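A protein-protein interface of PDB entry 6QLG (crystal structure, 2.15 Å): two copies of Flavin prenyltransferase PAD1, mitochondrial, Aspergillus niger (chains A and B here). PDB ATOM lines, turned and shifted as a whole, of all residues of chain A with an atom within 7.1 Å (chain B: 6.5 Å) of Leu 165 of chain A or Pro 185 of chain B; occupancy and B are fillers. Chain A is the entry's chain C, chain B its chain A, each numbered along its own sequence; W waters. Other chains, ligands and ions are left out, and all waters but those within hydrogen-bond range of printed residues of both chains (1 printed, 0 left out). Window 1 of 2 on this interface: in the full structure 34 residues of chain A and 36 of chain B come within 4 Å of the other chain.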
ATOM      1  N   MET A 127      23.878   3.161 -32.924  1.00  0.00           N
ATOM      2  CA  MET A 127      22.727   3.943 -32.486  1.00  0.00           C
ATOM      3  C   MET A 127      21.509   3.652 -33.353  1.00  0.00           C
ATOM      4  O   MET A 127      20.374   3.658 -32.861  1.00  0.00           O
ATOM      5  CB  MET A 127      23.062   5.434 -32.510  1.00  0.00           C
ATOM      6  CG  MET A 127      24.177   5.832 -31.552  1.00  0.00           C
ATOM      7  SD  MET A 127      23.773   5.531 -29.817  1.00  0.00           S
ATOM      8  CE  MET A 127      24.625   3.987 -29.492  1.00  0.00           C
ATOM      9  N   LEU A 130      20.110   0.412 -32.015  1.00  0.00           N
ATOM     10  CA  LEU A 130      19.514   0.752 -30.725  1.00  0.00           C
ATOM     11  C   LEU A 130      18.148   1.401 -30.911  1.00  0.00           C
ATOM     12  O   LEU A 130      17.187   1.067 -30.205  1.00  0.00           O
ATOM     13  CB  LEU A 130      20.447   1.682 -29.946  1.00  0.00           C
ATOM     14  CG  LEU A 130      19.852   2.428 -28.748  1.00  0.00           C
ATOM     15  CD1 LEU A 130      19.337   1.452 -27.687  1.00  0.00           C
ATOM     16  CD2 LEU A 130      20.873   3.392 -28.151  1.00  0.00           C
ATOM     17  N   ALA A 160      26.083  -0.742 -26.847  1.00  0.00           N
ATOM     18  CA  ALA A 160      25.824   0.490 -27.588  1.00  0.00           C
ATOM     19  C   ALA A 160      27.052   1.389 -27.537  1.00  0.00           C
ATOM     20  O   ALA A 160      27.435   1.873 -26.467  1.00  0.00           O
ATOM     21  CB  ALA A 160      24.603   1.201 -27.015  1.00  0.00           C
ATOM     22  N   ARG A 161      27.662   1.627 -28.693  1.00  0.00           N
ATOM     23  CA  ARG A 161      28.904   2.387 -28.791  1.00  0.00           C
ATOM     24  C   ARG A 161      28.636   3.683 -29.545  1.00  0.00           C
ATOM     25  O   ARG A 161      28.319   3.660 -30.740  1.00  0.00           O
ATOM     26  CB  ARG A 161      29.990   1.560 -29.477  1.00  0.00           C
ATOM     27  CG  ARG A 161      31.395   2.117 -29.313  1.00  0.00           C
ATOM     28  CD  ARG A 161      31.757   3.011 -30.481  1.00  0.00           C
ATOM     29  NE  ARG A 161      32.889   3.882 -30.190  1.00  0.00           N
ATOM     30  CZ  ARG A 161      33.023   5.110 -30.678  1.00  0.00           C
ATOM     31  NH1 ARG A 161      34.083   5.842 -30.365  1.00  0.00           N
ATOM     32  NH2 ARG A 161      32.088   5.608 -31.475  1.00  0.00           N
ATOM     33  N   GLU A 162      28.777   4.808 -28.846  1.00  0.00           N
ATOM     34  CA  GLU A 162      28.664   6.134 -29.435  1.00  0.00           C
ATOM     35  C   GLU A 162      29.124   7.155 -28.408  1.00  0.00           C
ATOM     36  O   GLU A 162      28.884   6.980 -27.212  1.00  0.00           O
ATOM     37  CB  GLU A 162      27.224   6.437 -29.872  1.00  0.00           C
ATOM     38  CG  GLU A 162      27.011   7.833 -30.443  1.00  0.00           C
ATOM     39  CD  GLU A 162      27.705   8.036 -31.779  1.00  0.00           C
ATOM     40  OE1 GLU A 162      28.929   8.289 -31.788  1.00  0.00           O
ATOM     41  OE2 GLU A 162      27.025   7.943 -32.820  1.00  0.00           O
ATOM     42  N   THR A 163      29.791   8.214 -28.880  1.00  0.00           N
ATOM     43  CA  THR A 163      30.157   9.308 -27.993  1.00  0.00           C
ATOM     44  C   THR A 163      30.391  10.562 -28.819  1.00  0.00           C
ATOM     45  O   THR A 163      30.876  10.457 -29.954  1.00  0.00           O
ATOM     46  CB  THR A 163      31.402   8.968 -27.159  1.00  0.00           C
ATOM     47  OG1 THR A 163      31.559   9.937 -26.115  1.00  0.00           O
ATOM     48  CG2 THR A 163      32.668   8.929 -28.019  1.00  0.00           C
ATOM     49  N   PRO A 164      29.995  11.748 -28.327  1.00  0.00           N
ATOM     50  CA  PRO A 164      29.160  11.892 -27.128  1.00  0.00           C
ATOM     51  C   PRO A 164      27.726  11.451 -27.402  1.00  0.00           C
ATOM     52  O   PRO A 164      27.407  11.084 -28.533  1.00  0.00           O
ATOM     53  CB  PRO A 164      29.228  13.391 -26.825  1.00  0.00           C
ATOM     54  CG  PRO A 164      29.544  14.030 -28.137  1.00  0.00           C
ATOM     55  CD  PRO A 164      30.412  13.052 -28.875  1.00  0.00           C
ATOM     56  N   LEU A 165      26.875  11.477 -26.383  1.00  0.00           N
ATOM     57  CA  LEU A 165      25.501  11.013 -26.504  1.00  0.00           C
ATOM     58  C   LEU A 165      24.557  12.206 -26.546  1.00  0.00           C
ATOM     59  O   LEU A 165      24.703  13.148 -25.760  1.00  0.00           O
ATOM     60  CB  LEU A 165      25.135  10.085 -25.344  1.00  0.00           C
ATOM     61  CG  LEU A 165      25.954   8.794 -25.250  1.00  0.00           C
ATOM     62  CD1 LEU A 165      25.557   8.000 -24.017  1.00  0.00           C
ATOM     63  CD2 LEU A 165      25.795   7.952 -26.513  1.00  0.00           C
ATOM     64  N   SER A 166      23.604  12.167 -27.469  1.00  0.00           N
ATOM     65  CA  SER A 166      22.548  13.162 -27.527  1.00  0.00           C
ATOM     66  C   SER A 166      21.392  12.743 -26.624  1.00  0.00           C
ATOM     67  O   SER A 166      21.379  11.651 -26.052  1.00  0.00           O
ATOM     68  CB  SER A 166      22.054  13.343 -28.961  1.00  0.00           C
ATOM     69  OG  SER A 166      21.145  12.309 -29.306  1.00  0.00           O
ATOM     70  N   GLU A 167      20.403  13.632 -26.505  1.00  0.00           N
ATOM     71  CA  GLU A 167      19.197  13.288 -25.762  1.00  0.00           C
ATOM     72  C   GLU A 167      18.436  12.147 -26.431  1.00  0.00           C
ATOM     73  O   GLU A 167      17.760  11.369 -25.749  1.00  0.00           O
ATOM     74  CB  GLU A 167      18.299  14.518 -25.619  1.00  0.00           C
ATOM     75  CG  GLU A 167      17.216  14.362 -24.570  1.00  0.00           C
ATOM     76  CD  GLU A 167      16.019  15.256 -24.818  1.00  0.00           C
ATOM     77  OE1 GLU A 167      14.882  14.741 -24.777  1.00  0.00           O
ATOM     78  OE2 GLU A 167      16.213  16.471 -25.043  1.00  0.00           O
ATOM     79  N   ILE A 168      18.537  12.033 -27.758  1.00  0.00           N
ATOM     80  CA  ILE A 168      17.894  10.929 -28.470  1.00  0.00           C
ATOM     81  C   ILE A 168      18.505   9.599 -28.048  1.00  0.00           C
ATOM     82  O   ILE A 168      17.792   8.640 -27.726  1.00  0.00           O
ATOM     83  CB  ILE A 168      18.004  11.131 -29.992  1.00  0.00           C
ATOM     84  CG1 ILE A 168      17.422  12.484 -30.406  1.00  0.00           C
ATOM     85  CG2 ILE A 168      17.313   9.994 -30.729  1.00  0.00           C
ATOM     86  CD1 ILE A 168      15.956  12.619 -30.123  1.00  0.00           C
ATOM     87  N   HIS A 169      19.839   9.518 -28.062  1.00  0.00           N
ATOM     88  CA  HIS A 169      20.519   8.286 -27.675  1.00  0.00           C
ATOM     89  C   HIS A 169      20.157   7.882 -26.250  1.00  0.00           C
ATOM     90  O   HIS A 169      19.844   6.716 -25.983  1.00  0.00           O
ATOM     91  CB  HIS A 169      22.035   8.455 -27.808  1.00  0.00           C
ATOM     92  CG  HIS A 169      22.487   8.885 -29.170  1.00  0.00           C
ATOM     93  ND1 HIS A 169      23.515   9.782 -29.362  1.00  0.00           N
ATOM     94  CD2 HIS A 169      22.061   8.533 -30.406  1.00  0.00           C
ATOM     95  CE1 HIS A 169      23.701   9.968 -30.656  1.00  0.00           C
ATOM     96  NE2 HIS A 169      22.833   9.220 -31.313  1.00  0.00           N
ATOM     97  N   LEU A 170      20.194   8.839 -25.320  1.00  0.00           N
ATOM     98  CA  LEU A 170      19.984   8.511 -23.911  1.00  0.00           C
ATOM     99  C   LEU A 170      18.530   8.145 -23.633  1.00  0.00           C
ATOM    100  O   LEU A 170      18.254   7.252 -22.820  1.00  0.00           O
ATOM    101  CB  LEU A 170      20.434   9.678 -23.035  1.00  0.00           C
ATOM    102  CG  LEU A 170      21.957   9.812 -22.939  1.00  0.00           C
ATOM    103  CD1 LEU A 170      22.361  11.178 -22.418  1.00  0.00           C
ATOM    104  CD2 LEU A 170      22.525   8.712 -22.059  1.00  0.00           C
ATOM    105  N   MET A 173      18.258   4.611 -24.765  1.00  0.00           N
ATOM    106  CA  MET A 173      18.919   3.710 -23.824  1.00  0.00           C
ATOM    107  C   MET A 173      18.083   3.515 -22.567  1.00  0.00           C
ATOM    108  O   MET A 173      17.912   2.386 -22.091  1.00  0.00           O
ATOM    109  CB  MET A 173      20.300   4.254 -23.460  1.00  0.00           C
ATOM    110  CG  MET A 173      21.303   4.223 -24.590  1.00  0.00           C
ATOM    111  SD  MET A 173      22.858   4.987 -24.103  1.00  0.00           S
ATOM    112  CE  MET A 173      23.832   4.728 -25.591  1.00  0.00           C
ATOM    113  N   PRO A 185      27.916   0.007 -22.581  1.00  0.00           N
ATOM    114  CA  PRO A 185      28.904   0.784 -23.334  1.00  0.00           C
ATOM    115  C   PRO A 185      30.281   0.175 -23.162  1.00  0.00           C
ATOM    116  O   PRO A 185      30.698  -0.122 -22.032  1.00  0.00           O
ATOM    117  CB  PRO A 185      28.824   2.185 -22.709  1.00  0.00           C
ATOM    118  CG  PRO A 185      28.206   1.986 -21.373  1.00  0.00           C
ATOM    119  CD  PRO A 185      27.373   0.743 -21.427  1.00  0.00           C
ATOM    120  N   VAL A 187      33.339   0.653 -22.424  1.00  0.00           N
ATOM    121  CA  VAL A 187      34.320   1.576 -21.858  1.00  0.00           C
ATOM    122  C   VAL A 187      35.436   0.773 -21.195  1.00  0.00           C
ATOM    123  O   VAL A 187      35.161  -0.177 -20.447  1.00  0.00           O
ATOM    124  CB  VAL A 187      33.665   2.558 -20.872  1.00  0.00           C
ATOM    125  CG1 VAL A 187      32.812   3.569 -21.626  1.00  0.00           C
ATOM    126  CG2 VAL A 187      32.823   1.815 -19.842  1.00  0.00           C
ATOM    127  N   LEU B 158      30.797  15.668 -19.120  1.00  0.00           N
ATOM    128  CA  LEU B 158      30.978  14.607 -18.136  1.00  0.00           C
ATOM    129  C   LEU B 158      31.428  13.350 -18.868  1.00  0.00           C
ATOM    130  O   LEU B 158      30.639  12.729 -19.589  1.00  0.00           O
ATOM    131  CB  LEU B 158      29.688  14.351 -17.359  1.00  0.00           C
ATOM    132  CG  LEU B 158      28.977  15.550 -16.732  1.00  0.00           C
ATOM    133  CD1 LEU B 158      27.735  15.091 -15.986  1.00  0.00           C
ATOM    134  CD2 LEU B 158      29.910  16.301 -15.802  1.00  0.00           C
ATOM    135  N   VAL B 159      32.692  12.974 -18.682  1.00  0.00           N
ATOM    136  CA  VAL B 159      33.204  11.726 -19.239  1.00  0.00           C
ATOM    137  C   VAL B 159      32.779  10.589 -18.317  1.00  0.00           C
ATOM    138  O   VAL B 159      33.602  10.008 -17.599  1.00  0.00           O
ATOM    139  CB  VAL B 159      34.733  11.781 -19.428  1.00  0.00           C
ATOM    140  CG1 VAL B 159      35.230  10.557 -20.190  1.00  0.00           C
ATOM    141  CG2 VAL B 159      35.121  13.055 -20.170  1.00  0.00           C
ATOM    142  N   ALA B 160      31.483  10.274 -18.331  1.00  0.00           N
ATOM    143  CA  ALA B 160      30.901   9.329 -17.383  1.00  0.00           C
ATOM    144  C   ALA B 160      31.279   7.905 -17.769  1.00  0.00           C
ATOM    145  O   ALA B 160      30.898   7.425 -18.842  1.00  0.00           O
ATOM    146  CB  ALA B 160      29.382   9.489 -17.342  1.00  0.00           C
ATOM    147  N   ARG B 161      32.011   7.223 -16.894  1.00  0.00           N
ATOM    148  CA  ARG B 161      32.546   5.898 -17.185  1.00  0.00           C
ATOM    149  C   ARG B 161      31.913   4.883 -16.243  1.00  0.00           C
ATOM    150  O   ARG B 161      32.108   4.950 -15.023  1.00  0.00           O
ATOM    151  CB  ARG B 161      34.068   5.890 -17.063  1.00  0.00           C
ATOM    152  CG  ARG B 161      34.712   4.668 -17.680  1.00  0.00           C
ATOM    153  CD  ARG B 161      34.935   3.586 -16.642  1.00  0.00           C
ATOM    154  NE  ARG B 161      35.221   2.291 -17.253  1.00  0.00           N
ATOM    155  CZ  ARG B 161      34.812   1.128 -16.755  1.00  0.00           C
ATOM    156  NH1 ARG B 161      35.108  -0.006 -17.377  1.00  0.00           N
ATOM    157  NH2 ARG B 161      34.098   1.098 -15.639  1.00  0.00           N
ATOM    158  N   LEU B 165      25.170  -0.221 -17.574  1.00  0.00           N
ATOM    159  CA  LEU B 165      24.440   0.889 -16.982  1.00  0.00           C
ATOM    160  C   LEU B 165      23.096   0.409 -16.454  1.00  0.00           C
ATOM    161  O   LEU B 165      22.409  -0.386 -17.102  1.00  0.00           O
ATOM    162  CB  LEU B 165      24.226   2.013 -18.000  1.00  0.00           C
ATOM    163  CG  LEU B 165      25.475   2.685 -18.573  1.00  0.00           C
ATOM    164  CD1 LEU B 165      25.079   3.739 -19.593  1.00  0.00           C
ATOM    165  CD2 LEU B 165      26.323   3.294 -17.463  1.00  0.00           C
ATOM    166  N   LEU B 170      21.233   5.767 -16.309  1.00  0.00           N
ATOM    167  CA  LEU B 170      20.706   6.306 -17.558  1.00  0.00           C
ATOM    168  C   LEU B 170      19.741   7.456 -17.305  1.00  0.00           C
ATOM    169  O   LEU B 170      19.726   8.435 -18.061  1.00  0.00           O
ATOM    170  CB  LEU B 170      20.032   5.193 -18.362  1.00  0.00           C
ATOM    171  CG  LEU B 170      21.046   4.311 -19.094  1.00  0.00           C
ATOM    172  CD1 LEU B 170      20.392   3.075 -19.676  1.00  0.00           C
ATOM    173  CD2 LEU B 170      21.746   5.117 -20.183  1.00  0.00           C
ATOM    174  N   MET B 173      21.895  10.403 -16.567  1.00  0.00           N
ATOM    175  CA  MET B 173      22.515  10.905 -17.791  1.00  0.00           C
ATOM    176  C   MET B 173      21.516  11.678 -18.641  1.00  0.00           C
ATOM    177  O   MET B 173      21.815  12.780 -19.118  1.00  0.00           O
ATOM    178  CB  MET B 173      23.106   9.747 -18.595  1.00  0.00           C
ATOM    179  CG  MET B 173      24.379   9.157 -18.016  1.00  0.00           C
ATOM    180  SD  MET B 173      24.881   7.688 -18.929  1.00  0.00           S
ATOM    181  CE  MET B 173      26.268   7.136 -17.935  1.00  0.00           C
ATOM    182  N   THR B 177      21.595  15.743 -19.048  1.00  0.00           N
ATOM    183  CA  THR B 177      21.738  16.222 -20.420  1.00  0.00           C
ATOM    184  C   THR B 177      20.711  17.307 -20.720  1.00  0.00           C
ATOM    185  O   THR B 177      21.040  18.357 -21.283  1.00  0.00           O
ATOM    186  CB  THR B 177      21.596  15.055 -21.402  1.00  0.00           C
ATOM    187  OG1 THR B 177      22.772  14.238 -21.361  1.00  0.00           O
ATOM    188  CG2 THR B 177      21.382  15.561 -22.825  1.00  0.00           C
ATOM    189  N   ALA B 181      24.168  19.461 -19.596  1.00  0.00           N
ATOM    190  CA  ALA B 181      25.460  18.790 -19.620  1.00  0.00           C
ATOM    191  C   ALA B 181      25.583  17.890 -20.848  1.00  0.00           C
ATOM    192  O   ALA B 181      24.595  17.537 -21.497  1.00  0.00           O
ATOM    193  CB  ALA B 181      25.669  17.968 -18.349  1.00  0.00           C
ATOM    194  N   VAL B 182      26.822  17.520 -21.161  1.00  0.00           N
ATOM    195  CA  VAL B 182      27.130  16.624 -22.271  1.00  0.00           C
ATOM    196  C   VAL B 182      27.738  15.352 -21.697  1.00  0.00           C
ATOM    197  O   VAL B 182      28.770  15.402 -21.016  1.00  0.00           O
ATOM    198  CB  VAL B 182      28.083  17.278 -23.283  1.00  0.00           C
ATOM    199  CG1 VAL B 182      28.439  16.289 -24.390  1.00  0.00           C
ATOM    200  CG2 VAL B 182      27.462  18.543 -23.862  1.00  0.00           C
ATOM    201  N   ILE B 183      27.104  14.217 -21.973  1.00  0.00           N
ATOM    202  CA  ILE B 183      27.605  12.916 -21.540  1.00  0.00           C
ATOM    203  C   ILE B 183      28.550  12.383 -22.613  1.00  0.00           C
ATOM    204  O   ILE B 183      28.153  12.212 -23.770  1.00  0.00           O
ATOM    205  CB  ILE B 183      26.453  11.932 -21.282  1.00  0.00           C
ATOM    206  CG1 ILE B 183      25.482  12.499 -20.243  1.00  0.00           C
ATOM    207  CG2 ILE B 183      26.993  10.576 -20.836  1.00  0.00           C
ATOM    208  CD1 ILE B 183      26.116  12.765 -18.889  1.00  0.00           C
ATOM    209  N   PHE B 184      29.801  12.118 -22.229  1.00  0.00           N
ATOM    210  CA  PHE B 184      30.835  11.628 -23.141  1.00  0.00           C
ATOM    211  C   PHE B 184      31.392  10.322 -22.588  1.00  0.00           C
ATOM    212  O   PHE B 184      32.419  10.322 -21.892  1.00  0.00           O
ATOM    213  CB  PHE B 184      31.946  12.666 -23.324  1.00  0.00           C
ATOM    214  CG  PHE B 184      32.894  12.368 -24.469  1.00  0.00           C
ATOM    215  CD1 PHE B 184      33.816  11.333 -24.386  1.00  0.00           C
ATOM    216  CD2 PHE B 184      32.869  13.137 -25.622  1.00  0.00           C
ATOM    217  CE1 PHE B 184      34.683  11.062 -25.434  1.00  0.00           C
ATOM    218  CE2 PHE B 184      33.736  12.872 -26.674  1.00  0.00           C
ATOM    219  CZ  PHE B 184      34.643  11.833 -26.578  1.00  0.00           C
ATOM    220  N   PRO B 185      30.758   9.189 -22.867  1.00  0.00           N
ATOM    221  CA  PRO B 185      31.349   7.903 -22.483  1.00  0.00           C
ATOM    222  C   PRO B 185      32.631   7.661 -23.257  1.00  0.00           C
ATOM    223  O   PRO B 185      32.661   7.812 -24.487  1.00  0.00           O
ATOM    224  CB  PRO B 185      30.263   6.881 -22.853  1.00  0.00           C
ATOM    225  CG  PRO B 185      29.385   7.573 -23.834  1.00  0.00           C
ATOM    226  CD  PRO B 185      29.458   9.038 -23.543  1.00  0.00           C
ATOM    227  N   PRO B 186      33.718   7.306 -22.574  1.00  0.00           N
ATOM    228  CA  PRO B 186      35.015   7.157 -23.268  1.00  0.00           C
ATOM    229  C   PRO B 186      35.140   5.819 -23.988  1.00  0.00           C
ATOM    230  O   PRO B 186      35.936   4.944 -23.634  1.00  0.00           O
ATOM    231  CB  PRO B 186      36.016   7.311 -22.118  1.00  0.00           C
ATOM    232  CG  PRO B 186      35.300   6.734 -20.936  1.00  0.00           C
ATOM    233  CD  PRO B 186      33.834   7.080 -21.122  1.00  0.00           C
ATOM    234  N   VAL B 187      34.331   5.644 -25.031  1.00  0.00           N
ATOM    235  CA  VAL B 187      34.346   4.411 -25.815  1.00  0.00           C
ATOM    236  C   VAL B 187      35.377   4.551 -26.931  1.00  0.00           C
ATOM    237  O   VAL B 187      35.416   5.584 -27.616  1.00  0.00           O
ATOM    238  CB  VAL B 187      32.950   4.074 -26.370  1.00  0.00           C
ATOM    239  CG1 VAL B 187      32.034   3.593 -25.247  1.00  0.00           C
ATOM    240  CG2 VAL B 187      32.339   5.275 -27.084  1.00  0.00           C
ATOM    241  N   PRO B 188      36.223   3.544 -27.149  1.00  0.00           N
ATOM    242  CA  PRO B 188      37.324   3.697 -28.111  1.00  0.00           C
ATOM    243  C   PRO B 188      36.822   3.754 -29.545  1.00  0.00           C
ATOM    244  O   PRO B 188      35.864   3.073 -29.917  1.00  0.00           O
ATOM    245  CB  PRO B 188      38.181   2.445 -27.876  1.00  0.00           C
ATOM    246  CG  PRO B 188      37.642   1.805 -26.621  1.00  0.00           C
ATOM    247  CD  PRO B 188      36.214   2.214 -26.525  1.00  0.00           C
ATOM    248  N   SER B 204      40.195   9.988 -28.152  1.00  0.00           N
ATOM    249  CA  SER B 204      39.114  10.337 -27.235  1.00  0.00           C
ATOM    250  C   SER B 204      39.319  11.727 -26.647  1.00  0.00           C
ATOM    251  O   SER B 204      38.372  12.517 -26.561  1.00  0.00           O
ATOM    252  CB  SER B 204      39.012   9.300 -26.117  1.00  0.00           C
ATOM    253  OG  SER B 204      38.672   8.022 -26.626  1.00  0.00           O
HETATM  254  O   HOH W   1      24.701  14.274 -23.350  1.00  0.00           O
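Water W1 lies within hydrogen-bond range of the backbone carbonyl oxygen of Leu 165 of chain A (2.7 Å), the backbone NH of Ile 183 of chain B (2.8 Å) and the side-chain hydroxyl of Thr 177 of chain B (2.8 Å).
Arg 161 of chain A touches Val 187 of chain B, and with the chains exchanged Val 187 of chain A touches Arg 161 of chain B. Leu 165 of chain A touches Pro 185 of chain B, and with the chains exchanged Pro 185 of chain A touches Leu 165 of chain B. Leu 170 of chain A touches Met 173 of chain B, and with the chains exchanged Met 173 of chain A touches Leu 170 of chain B. Val 187 of chain B touches its own counterpart, Val 187 of chain A. Of the 19 pairs that touch across the chains among the printed residues, 7 have their exchanged pair printed and touching as well.
Among the printed residues, pairs that only touch across the chains: Glu 162 of chain A with Pro 185 of chain B (3.5 Å), Glu 162 of chain A with Val 187 of chain B (3.9 Å), Thr 163 of chain A with Phe 184 of chain B (3.2 Å), Thr 163 of chain A with Val 187 of chain B (3.8 Å), Pro 164 of chain A with Val 182 of chain B (3.9 Å), Pro 164 of chain A with Ile 183 of chain B (3.4 Å), Pro 164 of chain A with Phe 184 of chain B (3.8 Å), Leu 165 of chain A with Pro 185 of chain B (3.9 Å), Leu 170 of chain A with Met 173 of chain B (3.7 Å), Leu 170 of chain A with Thr 177 of chain B (3.3 Å), Met 173 of chain A with Leu 170 of chain B (3.5 Å), Pro 185 of chain A with Leu 165 of chain B (3.9 Å), Val 187 of chain A with Pro 186 of chain B (3.7 Å) and Val 187 of chain A with Val 187 of chain B (3.7 Å).
Hydrophobic or aromatic side chains of chain A that line the printed part of chain B: Pro 164, Leu 165, Leu 170, Met 173, Pro 185 and Val 187. Of the 17 printed residues of chain B, 12 touch a printed residue of chain A. Along chain B the printed residues that touch a printed residue of chain A span positions 161 to 188.
The guanidinium group (NH1) of Arg 161 of chain B is in hydrogen-bond range of the backbone carbonyl oxygen (O) of Val 187 of chain A (3.1 Å). The backbone carbonyl oxygen of Pro 185 of chain B lies within hydrogen-bond range of the side-chain hydroxyl of Thr 163 of chain A (2.9 Å). NE of Arg 161 of chain A is in hydrogen-bond range of O of Pro 188 of chain B, at 3.1 Å. The backbone NH of Leu 165 of chain A sits at hydrogen-bond distance from the backbone carbonyl oxygen of Ile 183 of chain B (3.0 Å). The backbone carbonyl oxygen (O) of Val 187 of chain B sits at hydrogen-bond distance from the guanidinium group (NH1) of Arg 161 of chain A (3.1 Å).
The backbone carbonyl oxygen of Val 182 of chain B lies within hydrogen-bond range of the backbone NH of Leu 158 of chain B (2.8 Å). O of Met 173 of chain B is in hydrogen-bond range of OG1 of Thr 177 of chain B. N of Phe 184 of chain B sits at hydrogen-bond distance from O of Leu 158 of chain B (2.8 Å).
Leu 165 of chain A touches two residues of chain B. Pro 185 of chain B touches just these residues of chain A: Glu 162, Thr 163 and Leu 165. Printed residues of chain A within 4 Å of Thr 177 of chain B: Leu 170 (3.3 Å). Printed residues of chain B within 4 Å of Leu 170 of chain A: Met 173 (3.7 Å) and Thr 177 (3.3 Å). Ala 160 of chain A touches none of the printed residues of chain B.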
